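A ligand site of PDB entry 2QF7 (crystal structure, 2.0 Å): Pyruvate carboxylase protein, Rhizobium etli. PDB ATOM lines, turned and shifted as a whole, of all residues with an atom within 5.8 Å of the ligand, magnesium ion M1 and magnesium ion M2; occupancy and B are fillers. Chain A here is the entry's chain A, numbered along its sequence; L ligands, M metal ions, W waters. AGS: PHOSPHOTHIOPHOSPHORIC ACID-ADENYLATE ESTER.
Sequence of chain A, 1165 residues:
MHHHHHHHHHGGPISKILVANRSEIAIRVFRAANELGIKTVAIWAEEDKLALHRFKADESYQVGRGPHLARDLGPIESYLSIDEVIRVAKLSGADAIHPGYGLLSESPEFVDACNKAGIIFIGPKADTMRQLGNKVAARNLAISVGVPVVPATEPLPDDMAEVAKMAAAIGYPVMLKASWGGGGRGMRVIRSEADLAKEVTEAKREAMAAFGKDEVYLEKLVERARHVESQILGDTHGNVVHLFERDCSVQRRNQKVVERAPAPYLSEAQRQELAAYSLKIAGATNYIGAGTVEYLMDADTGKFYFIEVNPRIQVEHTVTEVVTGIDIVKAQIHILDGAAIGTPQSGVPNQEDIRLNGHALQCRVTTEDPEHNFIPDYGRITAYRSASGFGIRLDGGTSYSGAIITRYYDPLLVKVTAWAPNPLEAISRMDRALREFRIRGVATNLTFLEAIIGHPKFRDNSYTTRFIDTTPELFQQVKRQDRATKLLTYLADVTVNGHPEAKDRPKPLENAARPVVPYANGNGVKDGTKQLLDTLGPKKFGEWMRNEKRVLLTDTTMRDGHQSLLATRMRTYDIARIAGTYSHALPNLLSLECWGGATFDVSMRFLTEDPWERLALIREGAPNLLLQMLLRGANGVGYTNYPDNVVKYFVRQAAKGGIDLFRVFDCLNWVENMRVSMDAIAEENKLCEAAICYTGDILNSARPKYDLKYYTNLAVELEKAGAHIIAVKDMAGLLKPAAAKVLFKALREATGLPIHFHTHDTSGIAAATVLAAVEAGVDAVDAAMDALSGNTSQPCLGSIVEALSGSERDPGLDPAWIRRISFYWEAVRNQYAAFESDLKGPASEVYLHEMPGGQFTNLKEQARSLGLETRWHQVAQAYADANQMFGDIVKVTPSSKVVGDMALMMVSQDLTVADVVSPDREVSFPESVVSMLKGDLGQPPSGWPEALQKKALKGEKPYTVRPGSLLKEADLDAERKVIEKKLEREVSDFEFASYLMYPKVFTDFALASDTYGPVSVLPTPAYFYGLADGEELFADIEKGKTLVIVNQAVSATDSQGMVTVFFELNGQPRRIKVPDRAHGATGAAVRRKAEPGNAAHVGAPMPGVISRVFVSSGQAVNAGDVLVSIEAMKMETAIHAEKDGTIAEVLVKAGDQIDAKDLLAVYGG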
ATOM      1  N   GLU A 106     -13.873   5.161 -21.123  1.00  0.00           N
ATOM      2  CA  GLU A 106     -15.289   5.273 -21.415  1.00  0.00           C
ATOM      3  C   GLU A 106     -15.626   4.858 -22.833  1.00  0.00           C
ATOM      4  O   GLU A 106     -16.668   5.281 -23.343  1.00  0.00           O
ATOM      5  CB  GLU A 106     -15.763   6.706 -21.273  1.00  0.00           C
ATOM      6  CG  GLU A 106     -15.729   7.284 -19.911  1.00  0.00           C
ATOM      7  CD  GLU A 106     -16.608   8.544 -19.860  1.00  0.00           C
ATOM      8  OE1 GLU A 106     -17.560   8.580 -19.062  1.00  0.00           O
ATOM      9  OE2 GLU A 106     -16.365   9.474 -20.660  1.00  0.00           O
ATOM     10  N   VAL A 150     -32.693  17.349 -13.122  1.00  0.00           N
ATOM     11  CA  VAL A 150     -32.860  18.819 -13.199  1.00  0.00           C
ATOM     12  C   VAL A 150     -34.241  19.244 -13.740  1.00  0.00           C
ATOM     13  O   VAL A 150     -34.629  18.830 -14.829  1.00  0.00           O
ATOM     14  CB  VAL A 150     -31.743  19.496 -14.026  1.00  0.00           C
ATOM     15  CG1 VAL A 150     -32.006  20.995 -14.161  1.00  0.00           C
ATOM     16  CG2 VAL A 150     -30.373  19.252 -13.396  1.00  0.00           C
ATOM     17  N   LYS A 220     -34.585  24.695 -14.685  1.00  0.00           N
ATOM     18  CA  LYS A 220     -34.252  25.225 -13.367  1.00  0.00           C
ATOM     19  C   LYS A 220     -32.892  25.883 -13.335  1.00  0.00           C
ATOM     20  O   LYS A 220     -32.021  25.537 -14.153  1.00  0.00           O
ATOM     21  CB  LYS A 220     -34.272  24.112 -12.309  1.00  0.00           C
ATOM     22  CG  LYS A 220     -35.646  23.750 -11.786  1.00  0.00           C
ATOM     23  CD  LYS A 220     -35.577  23.322 -10.334  1.00  0.00           C
ATOM     24  CE  LYS A 220     -35.977  24.451  -9.376  1.00  0.00           C
ATOM     25  NZ  LYS A 220     -34.923  25.480  -9.191  1.00  0.00           N
ATOM     26  N   LEU A 221     -32.735  26.850 -12.413  1.00  0.00           N
ATOM     27  CA  LEU A 221     -31.437  27.372 -11.914  1.00  0.00           C
ATOM     28  C   LEU A 221     -30.159  26.762 -12.608  1.00  0.00           C
ATOM     29  O   LEU A 221     -30.025  26.927 -13.837  1.00  0.00           O
ATOM     30  CB  LEU A 221     -31.444  27.272 -10.365  1.00  0.00           C
ATOM     31  CG  LEU A 221     -31.337  28.504  -9.425  1.00  0.00           C
ATOM     32  CD1 LEU A 221     -32.180  29.730  -9.876  1.00  0.00           C
ATOM     33  CD2 LEU A 221     -31.778  28.096  -8.015  1.00  0.00           C
ATOM     34  N   VAL A 222     -29.212  26.119 -11.926  1.00  0.00           N
ATOM     35  CA  VAL A 222     -28.929  26.218 -10.478  1.00  0.00           C
ATOM     36  C   VAL A 222     -27.795  27.213 -10.354  1.00  0.00           C
ATOM     37  O   VAL A 222     -26.683  26.947 -10.797  1.00  0.00           O
ATOM     38  CB  VAL A 222     -28.476  24.868  -9.863  1.00  0.00           C
ATOM     39  CG1 VAL A 222     -28.422  24.964  -8.339  1.00  0.00           C
ATOM     40  CG2 VAL A 222     -29.377  23.722 -10.305  1.00  0.00           C
ATOM     41  N   ALA A 225     -24.764  26.277  -6.828  1.00  0.00           N
ATOM     42  CA  ALA A 225     -24.712  24.839  -6.988  1.00  0.00           C
ATOM     43  C   ALA A 225     -23.533  24.218  -6.270  1.00  0.00           C
ATOM     44  O   ALA A 225     -22.459  24.793  -6.194  1.00  0.00           O
ATOM     45  CB  ALA A 225     -24.602  24.513  -8.461  1.00  0.00           C
ATOM     46  N   HIS A 227     -21.370  20.382  -6.451  1.00  0.00           N
ATOM     47  CA  HIS A 227     -21.232  19.099  -7.160  1.00  0.00           C
ATOM     48  C   HIS A 227     -20.915  18.026  -6.121  1.00  0.00           C
ATOM     49  O   HIS A 227     -19.888  18.089  -5.480  1.00  0.00           O
ATOM     50  CB  HIS A 227     -20.118  19.176  -8.228  1.00  0.00           C
ATOM     51  CG  HIS A 227     -19.747  17.843  -8.848  1.00  0.00           C
ATOM     52  ND1 HIS A 227     -19.916  17.572 -10.190  1.00  0.00           N
ATOM     53  CD2 HIS A 227     -19.163  16.733  -8.319  1.00  0.00           C
ATOM     54  CE1 HIS A 227     -19.479  16.356 -10.456  1.00  0.00           C
ATOM     55  NE2 HIS A 227     -19.020  15.820  -9.337  1.00  0.00           N
ATOM     56  N   CYS A 248     -17.078  17.844  -4.979  1.00  0.00           N
ATOM     57  CA  CYS A 248     -16.214  18.289  -6.046  1.00  0.00           C
ATOM     58  C   CYS A 248     -16.571  19.688  -6.536  1.00  0.00           C
ATOM     59  O   CYS A 248     -16.369  19.995  -7.692  1.00  0.00           O
ATOM     60  CB  CYS A 248     -16.271  17.280  -7.186  1.00  0.00           C
ATOM     61  SG  CYS A 248     -15.815  15.573  -6.711  1.00  0.00           S
ATOM     62  N   GLN A 251     -13.950  24.028  -8.416  1.00  0.00           N
ATOM     63  CA  GLN A 251     -13.649  23.857  -9.856  1.00  0.00           C
ATOM     64  C   GLN A 251     -13.191  25.199 -10.418  1.00  0.00           C
ATOM     65  O   GLN A 251     -13.718  26.243 -10.032  1.00  0.00           O
ATOM     66  CB  GLN A 251     -14.898  23.428 -10.636  1.00  0.00           C
ATOM     67  CG  GLN A 251     -15.826  22.533  -9.856  1.00  0.00           C
ATOM     68  CD  GLN A 251     -16.891  21.827 -10.682  1.00  0.00           C
ATOM     69  OE1 GLN A 251     -17.283  20.674 -10.382  1.00  0.00           O
ATOM     70  NE2 GLN A 251     -17.344  22.498 -11.745  1.00  0.00           N
ATOM     71  N   ASN A 254     -14.171  24.889 -15.735  1.00  0.00           N
ATOM     72  CA  ASN A 254     -15.063  23.774 -15.405  1.00  0.00           C
ATOM     73  C   ASN A 254     -14.349  22.496 -14.974  1.00  0.00           C
ATOM     74  O   ASN A 254     -14.933  21.398 -15.040  1.00  0.00           O
ATOM     75  CB  ASN A 254     -16.088  23.546 -16.524  1.00  0.00           C
ATOM     76  CG  ASN A 254     -17.432  24.281 -16.269  1.00  0.00           C
ATOM     77  OD1 ASN A 254     -17.473  25.487 -15.972  1.00  0.00           O
ATOM     78  ND2 ASN A 254     -18.534  23.533 -16.411  1.00  0.00           N
ATOM     79  N   LYS A 256     -12.114  20.147 -12.139  1.00  0.00           N
ATOM     80  CA  LYS A 256     -12.015  19.843 -10.688  1.00  0.00           C
ATOM     81  C   LYS A 256     -10.649  20.205 -10.147  1.00  0.00           C
ATOM     82  O   LYS A 256      -9.639  19.868 -10.773  1.00  0.00           O
ATOM     83  CB  LYS A 256     -12.259  18.349 -10.415  1.00  0.00           C
ATOM     84  CG  LYS A 256     -13.700  17.885 -10.568  1.00  0.00           C
ATOM     85  CD  LYS A 256     -13.828  16.425 -10.203  1.00  0.00           C
ATOM     86  CE  LYS A 256     -15.214  15.912 -10.568  1.00  0.00           C
ATOM     87  NZ  LYS A 256     -15.122  14.930 -11.685  1.00  0.00           N
ATOM     88  N   GLU A 294     -23.082  11.224 -10.267  1.00  0.00           N
ATOM     89  CA  GLU A 294     -22.879  12.650 -10.010  1.00  0.00           C
ATOM     90  C   GLU A 294     -24.186  13.396  -9.874  1.00  0.00           C
ATOM     91  O   GLU A 294     -25.109  13.203 -10.665  1.00  0.00           O
ATOM     92  CB  GLU A 294     -22.044  13.286 -11.124  1.00  0.00           C
ATOM     93  CG  GLU A 294     -20.756  12.483 -11.415  1.00  0.00           C
ATOM     94  CD  GLU A 294     -19.808  13.131 -12.398  1.00  0.00           C
ATOM     95  OE1 GLU A 294     -20.199  14.082 -13.139  1.00  0.00           O
ATOM     96  OE2 GLU A 294     -18.635  12.673 -12.440  1.00  0.00           O
ATOM     97  N   LEU A 296     -26.021  17.387  -8.889  1.00  0.00           N
ATOM     98  CA  LEU A 296     -26.001  18.761  -8.508  1.00  0.00           C
ATOM     99  C   LEU A 296     -26.892  18.924  -7.274  1.00  0.00           C
ATOM    100  O   LEU A 296     -27.989  18.358  -7.215  1.00  0.00           O
ATOM    101  CB  LEU A 296     -26.599  19.604  -9.629  1.00  0.00           C
ATOM    102  CG  LEU A 296     -25.697  20.788  -9.952  1.00  0.00           C
ATOM    103  CD1 LEU A 296     -25.090  20.598 -11.338  1.00  0.00           C
ATOM    104  CD2 LEU A 296     -26.537  21.999  -9.897  1.00  0.00           C
ATOM    105  N   ILE A 307     -27.110  14.060 -12.471  1.00  0.00           N
ATOM    106  CA  ILE A 307     -26.484  14.672 -13.640  1.00  0.00           C
ATOM    107  C   ILE A 307     -25.946  13.623 -14.620  1.00  0.00           C
ATOM    108  O   ILE A 307     -26.329  13.611 -15.792  1.00  0.00           O
ATOM    109  CB  ILE A 307     -25.347  15.691 -13.231  1.00  0.00           C
ATOM    110  CG1 ILE A 307     -25.952  16.867 -12.442  1.00  0.00           C
ATOM    111  CG2 ILE A 307     -24.615  16.221 -14.461  1.00  0.00           C
ATOM    112  N   GLU A 308     -25.071  12.720 -14.150  1.00  0.00           N
ATOM    113  CA  GLU A 308     -24.534  11.647 -15.012  1.00  0.00           C
ATOM    114  C   GLU A 308     -23.916  10.567 -14.131  1.00  0.00           C
ATOM    115  O   GLU A 308     -23.685  10.806 -12.953  1.00  0.00           O
ATOM    116  CB  GLU A 308     -23.446  12.189 -15.965  1.00  0.00           C
ATOM    117  CG  GLU A 308     -22.378  13.069 -15.304  1.00  0.00           C
ATOM    118  CD  GLU A 308     -21.092  13.160 -16.113  1.00  0.00           C
ATOM    119  OE1 GLU A 308     -21.088  12.641 -17.264  1.00  0.00           O
ATOM    120  OE2 GLU A 308     -20.070  13.691 -15.604  1.00  0.00           O
ATOM    121  N   VAL A 309     -23.713   9.377 -14.693  1.00  0.00           N
ATOM    122  CA  VAL A 309     -22.817   8.375 -14.094  1.00  0.00           C
ATOM    123  C   VAL A 309     -21.525   8.396 -14.885  1.00  0.00           C
ATOM    124  O   VAL A 309     -21.560   8.289 -16.108  1.00  0.00           O
ATOM    125  CB  VAL A 309     -23.384   6.935 -14.130  1.00  0.00           C
ATOM    126  CG1 VAL A 309     -22.326   5.916 -13.641  1.00  0.00           C
ATOM    127  CG2 VAL A 309     -24.666   6.827 -13.303  1.00  0.00           C
ATOM    128  N   ASN A 310     -20.394   8.550 -14.188  1.00  0.00           N
ATOM    129  CA  ASN A 310     -19.068   8.309 -14.772  1.00  0.00           C
ATOM    130  C   ASN A 310     -18.658   6.859 -14.601  1.00  0.00           C
ATOM    131  O   ASN A 310     -18.303   6.453 -13.495  1.00  0.00           O
ATOM    132  CB  ASN A 310     -18.030   9.198 -14.098  1.00  0.00           C
ATOM    133  CG  ASN A 310     -17.449  10.226 -15.027  1.00  0.00           C
ATOM    134  OD1 ASN A 310     -16.381  10.003 -15.613  1.00  0.00           O
ATOM    135  ND2 ASN A 310     -18.153  11.332 -15.203  1.00  0.00           N
ATOM    136  N   ARG A 312     -16.321   4.567 -14.522  1.00  0.00           N
ATOM    137  CA  ARG A 312     -14.892   4.316 -14.434  1.00  0.00           C
ATOM    138  C   ARG A 312     -14.441   4.823 -13.056  1.00  0.00           C
ATOM    139  O   ARG A 312     -15.175   5.570 -12.378  1.00  0.00           O
ATOM    140  CB  ARG A 312     -14.124   5.124 -15.518  1.00  0.00           C
ATOM    141  CG  ARG A 312     -14.620   6.578 -15.649  1.00  0.00           C
ATOM    142  CD  ARG A 312     -13.713   7.456 -16.480  1.00  0.00           C
ATOM    143  NE  ARG A 312     -14.044   8.887 -16.413  1.00  0.00           N
ATOM    144  CZ  ARG A 312     -13.561   9.791 -15.526  1.00  0.00           C
ATOM    145  NH1 ARG A 312     -12.734   9.461 -14.542  1.00  0.00           N
ATOM    146  NH2 ARG A 312     -13.954  11.059 -15.611  1.00  0.00           N
ATOM    147  N   GLN A 314     -12.105   7.337 -10.876  1.00  0.00           N
ATOM    148  CA  GLN A 314     -11.844   8.724 -11.083  1.00  0.00           C
ATOM    149  C   GLN A 314     -10.606   9.147 -10.324  1.00  0.00           C
ATOM    150  O   GLN A 314     -10.164   8.443  -9.413  1.00  0.00           O
ATOM    151  CB  GLN A 314     -13.006   9.570 -10.595  1.00  0.00           C
ATOM    152  CG  GLN A 314     -14.177   9.568 -11.587  1.00  0.00           C
ATOM    153  CD  GLN A 314     -15.327  10.314 -11.036  1.00  0.00           C
ATOM    154  OE1 GLN A 314     -15.770  10.026  -9.934  1.00  0.00           O
ATOM    155  NE2 GLN A 314     -15.790  11.328 -11.758  1.00  0.00           N
ATOM    156  N   THR A 465     -19.861  25.927  -7.055  1.00  0.00           N
ATOM    157  CA  THR A 465     -19.089  25.642  -8.270  1.00  0.00           C
ATOM    158  C   THR A 465     -18.543  26.912  -8.953  1.00  0.00           C
ATOM    159  O   THR A 465     -17.695  26.811  -9.838  1.00  0.00           O
ATOM    160  CB  THR A 465     -19.943  24.874  -9.290  1.00  0.00           C
ATOM    161  OG1 THR A 465     -21.139  25.627  -9.542  1.00  0.00           O
ATOM    162  CG2 THR A 465     -20.329  23.486  -8.743  1.00  0.00           C
HETATM  163  PG  AGS L   1     -17.124  15.516 -16.350  1.00  0.00           P
HETATM  164  S1G AGS L   1     -17.403  15.333 -14.429  1.00  0.00           S
HETATM  165  O2G AGS L   1     -17.432  13.973 -17.196  1.00  0.00           O
HETATM  166  O3G AGS L   1     -15.456  16.014 -16.697  1.00  0.00           O
HETATM  167  PB  AGS L   1     -19.069  16.545 -18.085  1.00  0.00           P
HETATM  168  O1B AGS L   1     -18.376  17.240 -19.234  1.00  0.00           O
HETATM  169  O2B AGS L   1     -19.532  15.117 -18.218  1.00  0.00           O
HETATM  170  O3B AGS L   1     -18.093  16.700 -16.836  1.00  0.00           O
HETATM  171  PA  AGS L   1     -21.073  17.444 -16.192  1.00  0.00           P
HETATM  172  O1A AGS L   1     -22.552  17.420 -16.504  1.00  0.00           O
HETATM  173  O2A AGS L   1     -20.489  16.347 -15.288  1.00  0.00           O
HETATM  174  O3A AGS L   1     -20.318  17.493 -17.640  1.00  0.00           O
HETATM  175  O5' AGS L   1     -20.661  18.849 -15.536  1.00  0.00           O
HETATM  176  C5' AGS L   1     -19.850  18.939 -14.352  1.00  0.00           C
HETATM  177  C4' AGS L   1     -19.877  20.383 -13.843  1.00  0.00           C
HETATM  178  O4' AGS L   1     -20.533  21.254 -14.787  1.00  0.00           O
HETATM  179  C3' AGS L   1     -20.640  20.546 -12.523  1.00  0.00           C
HETATM  180  O3' AGS L   1     -19.823  20.348 -11.354  1.00  0.00           O
HETATM  181  C2' AGS L   1     -21.144  21.968 -12.621  1.00  0.00           C
HETATM  182  O2' AGS L   1     -20.079  22.848 -12.222  1.00  0.00           O
HETATM  183  C1' AGS L   1     -21.394  22.181 -14.101  1.00  0.00           C
HETATM  184  N9  AGS L   1     -22.849  21.944 -14.423  1.00  0.00           N
HETATM  185  C8  AGS L   1     -23.372  20.917 -15.127  1.00  0.00           C
HETATM  186  N7  AGS L   1     -24.744  21.010 -15.230  1.00  0.00           N
HETATM  187  C5  AGS L   1     -25.107  22.130 -14.567  1.00  0.00           C
HETATM  188  C6  AGS L   1     -26.393  22.832 -14.280  1.00  0.00           C
HETATM  189  N6  AGS L   1     -27.581  22.360 -14.729  1.00  0.00           N
HETATM  190  N1  AGS L   1     -26.328  23.974 -13.550  1.00  0.00           N
HETATM  191  C2  AGS L   1     -25.151  24.493 -13.100  1.00  0.00           C
HETATM  192  N3  AGS L   1     -23.954  23.903 -13.325  1.00  0.00           N
HETATM  193  C4  AGS L   1     -23.865  22.743 -14.047  1.00  0.00           C
HETATM  194 MG    MG M   1     -19.290  14.802 -14.569  1.00  0.00          MG
HETATM  195 MG    MG M   2     -18.945  12.785 -18.062  1.00  0.00          MG
HETATM  196  O   HOH W   1     -14.883  14.189 -15.180  1.00  0.00           O
HETATM  197  O   HOH W   2     -22.267  25.553 -11.900  1.00  0.00           O
HETATM  198  O   HOH W   3     -16.134  18.023 -13.805  1.00  0.00           O
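Asn 310 touches magnesium ion M1 (ND2 to MG, 3.7 Å). Along chain A the residues within 4 Å of magnesium ion M1 span positions 294 to 310.
Residues that only touch magnesium ion M2: Asn 310 (3.3 Å). The nearest printed residue that does not touch magnesium ion M2 is Glu 106 (4.5 Å).
Magnesium ion M1 is bound by OE2 of Glu 308 (1.7 Å), OE1 of Glu 294 (1.8 Å), S1G of the ligand (2.0 Å) and O2A of the ligand (2.1 Å).
Water W1 bridges O3G of the ligand (2.4 Å) and NH2 of Arg 312 (3.3 Å). Water W2 lies within hydrogen-bond range of the side-chain hydroxyl (OG1) of Thr 465 (2.6 Å) and a nitrogen (N3) of the ligand (2.8 Å).
OE1 of Gln 251 sits at hydrogen-bond distance from O3' of the ligand (2.7 Å). O3' of the ligand lies within hydrogen-bond range of ND1 of His 227 (3.0 Å). An oxygen (O2G) of the ligand lies close to the side-chain amide nitrogen of Asn 310, 3.4 Å away. ND2 of Asn 254 sits at hydrogen-bond distance from O4' of the ligand, at 3.4 Å. A sulfur (S1G) of the ligand lies close to the side-chain amino group of Lys 256 (3.6 Å).
An oxygen (O2G) of the ligand binds magnesium ion M2 (2.1 Å). OE1 of Glu 308 binds magnesium ion M2 (2.3 Å). O2B of the ligand is bound to magnesium ion M2 (2.4 Å).
Merely in contact with the ligand: Val 222 (3.7 Å), Leu 296 (3.6 Å), Ile 307 (3.1 Å) and Thr 465 (3.5 Å). Within 4 Å of the ligand: Val 222, His 227, Gln 251, Asn 254, Lys 256, Glu 294, Leu 296, Ile 307, Glu 308, Asn 310 and Thr 465.
OE2 of Glu 308 sits close to ND2 of Asn 310. O of Glu 294 is in hydrogen-bond range of N of Ile 307 (2.8 Å). ND2 of Asn 310 lies within hydrogen-bond range of OE2 of Glu 294, at 3.1 Å. The side-chain amide nitrogen of Gln 314 lies within hydrogen-bond range of the side-chain carboxylate of Glu 294 (3.2 Å). The side-chain amide oxygen of Gln 251 sits close to the backbone carbonyl oxygen of Cys 248, at 2.9 Å. The backbone NH (N) of Cys 248 sits at hydrogen-bond distance from the backbone carbonyl oxygen (O) of His 227. OD1 of Asn 310 lies within hydrogen-bond range of NH2 of Arg 312 (2.6 Å). N of Thr 465 is in hydrogen-bond range of O of Ala 225, 3.0 Å away.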
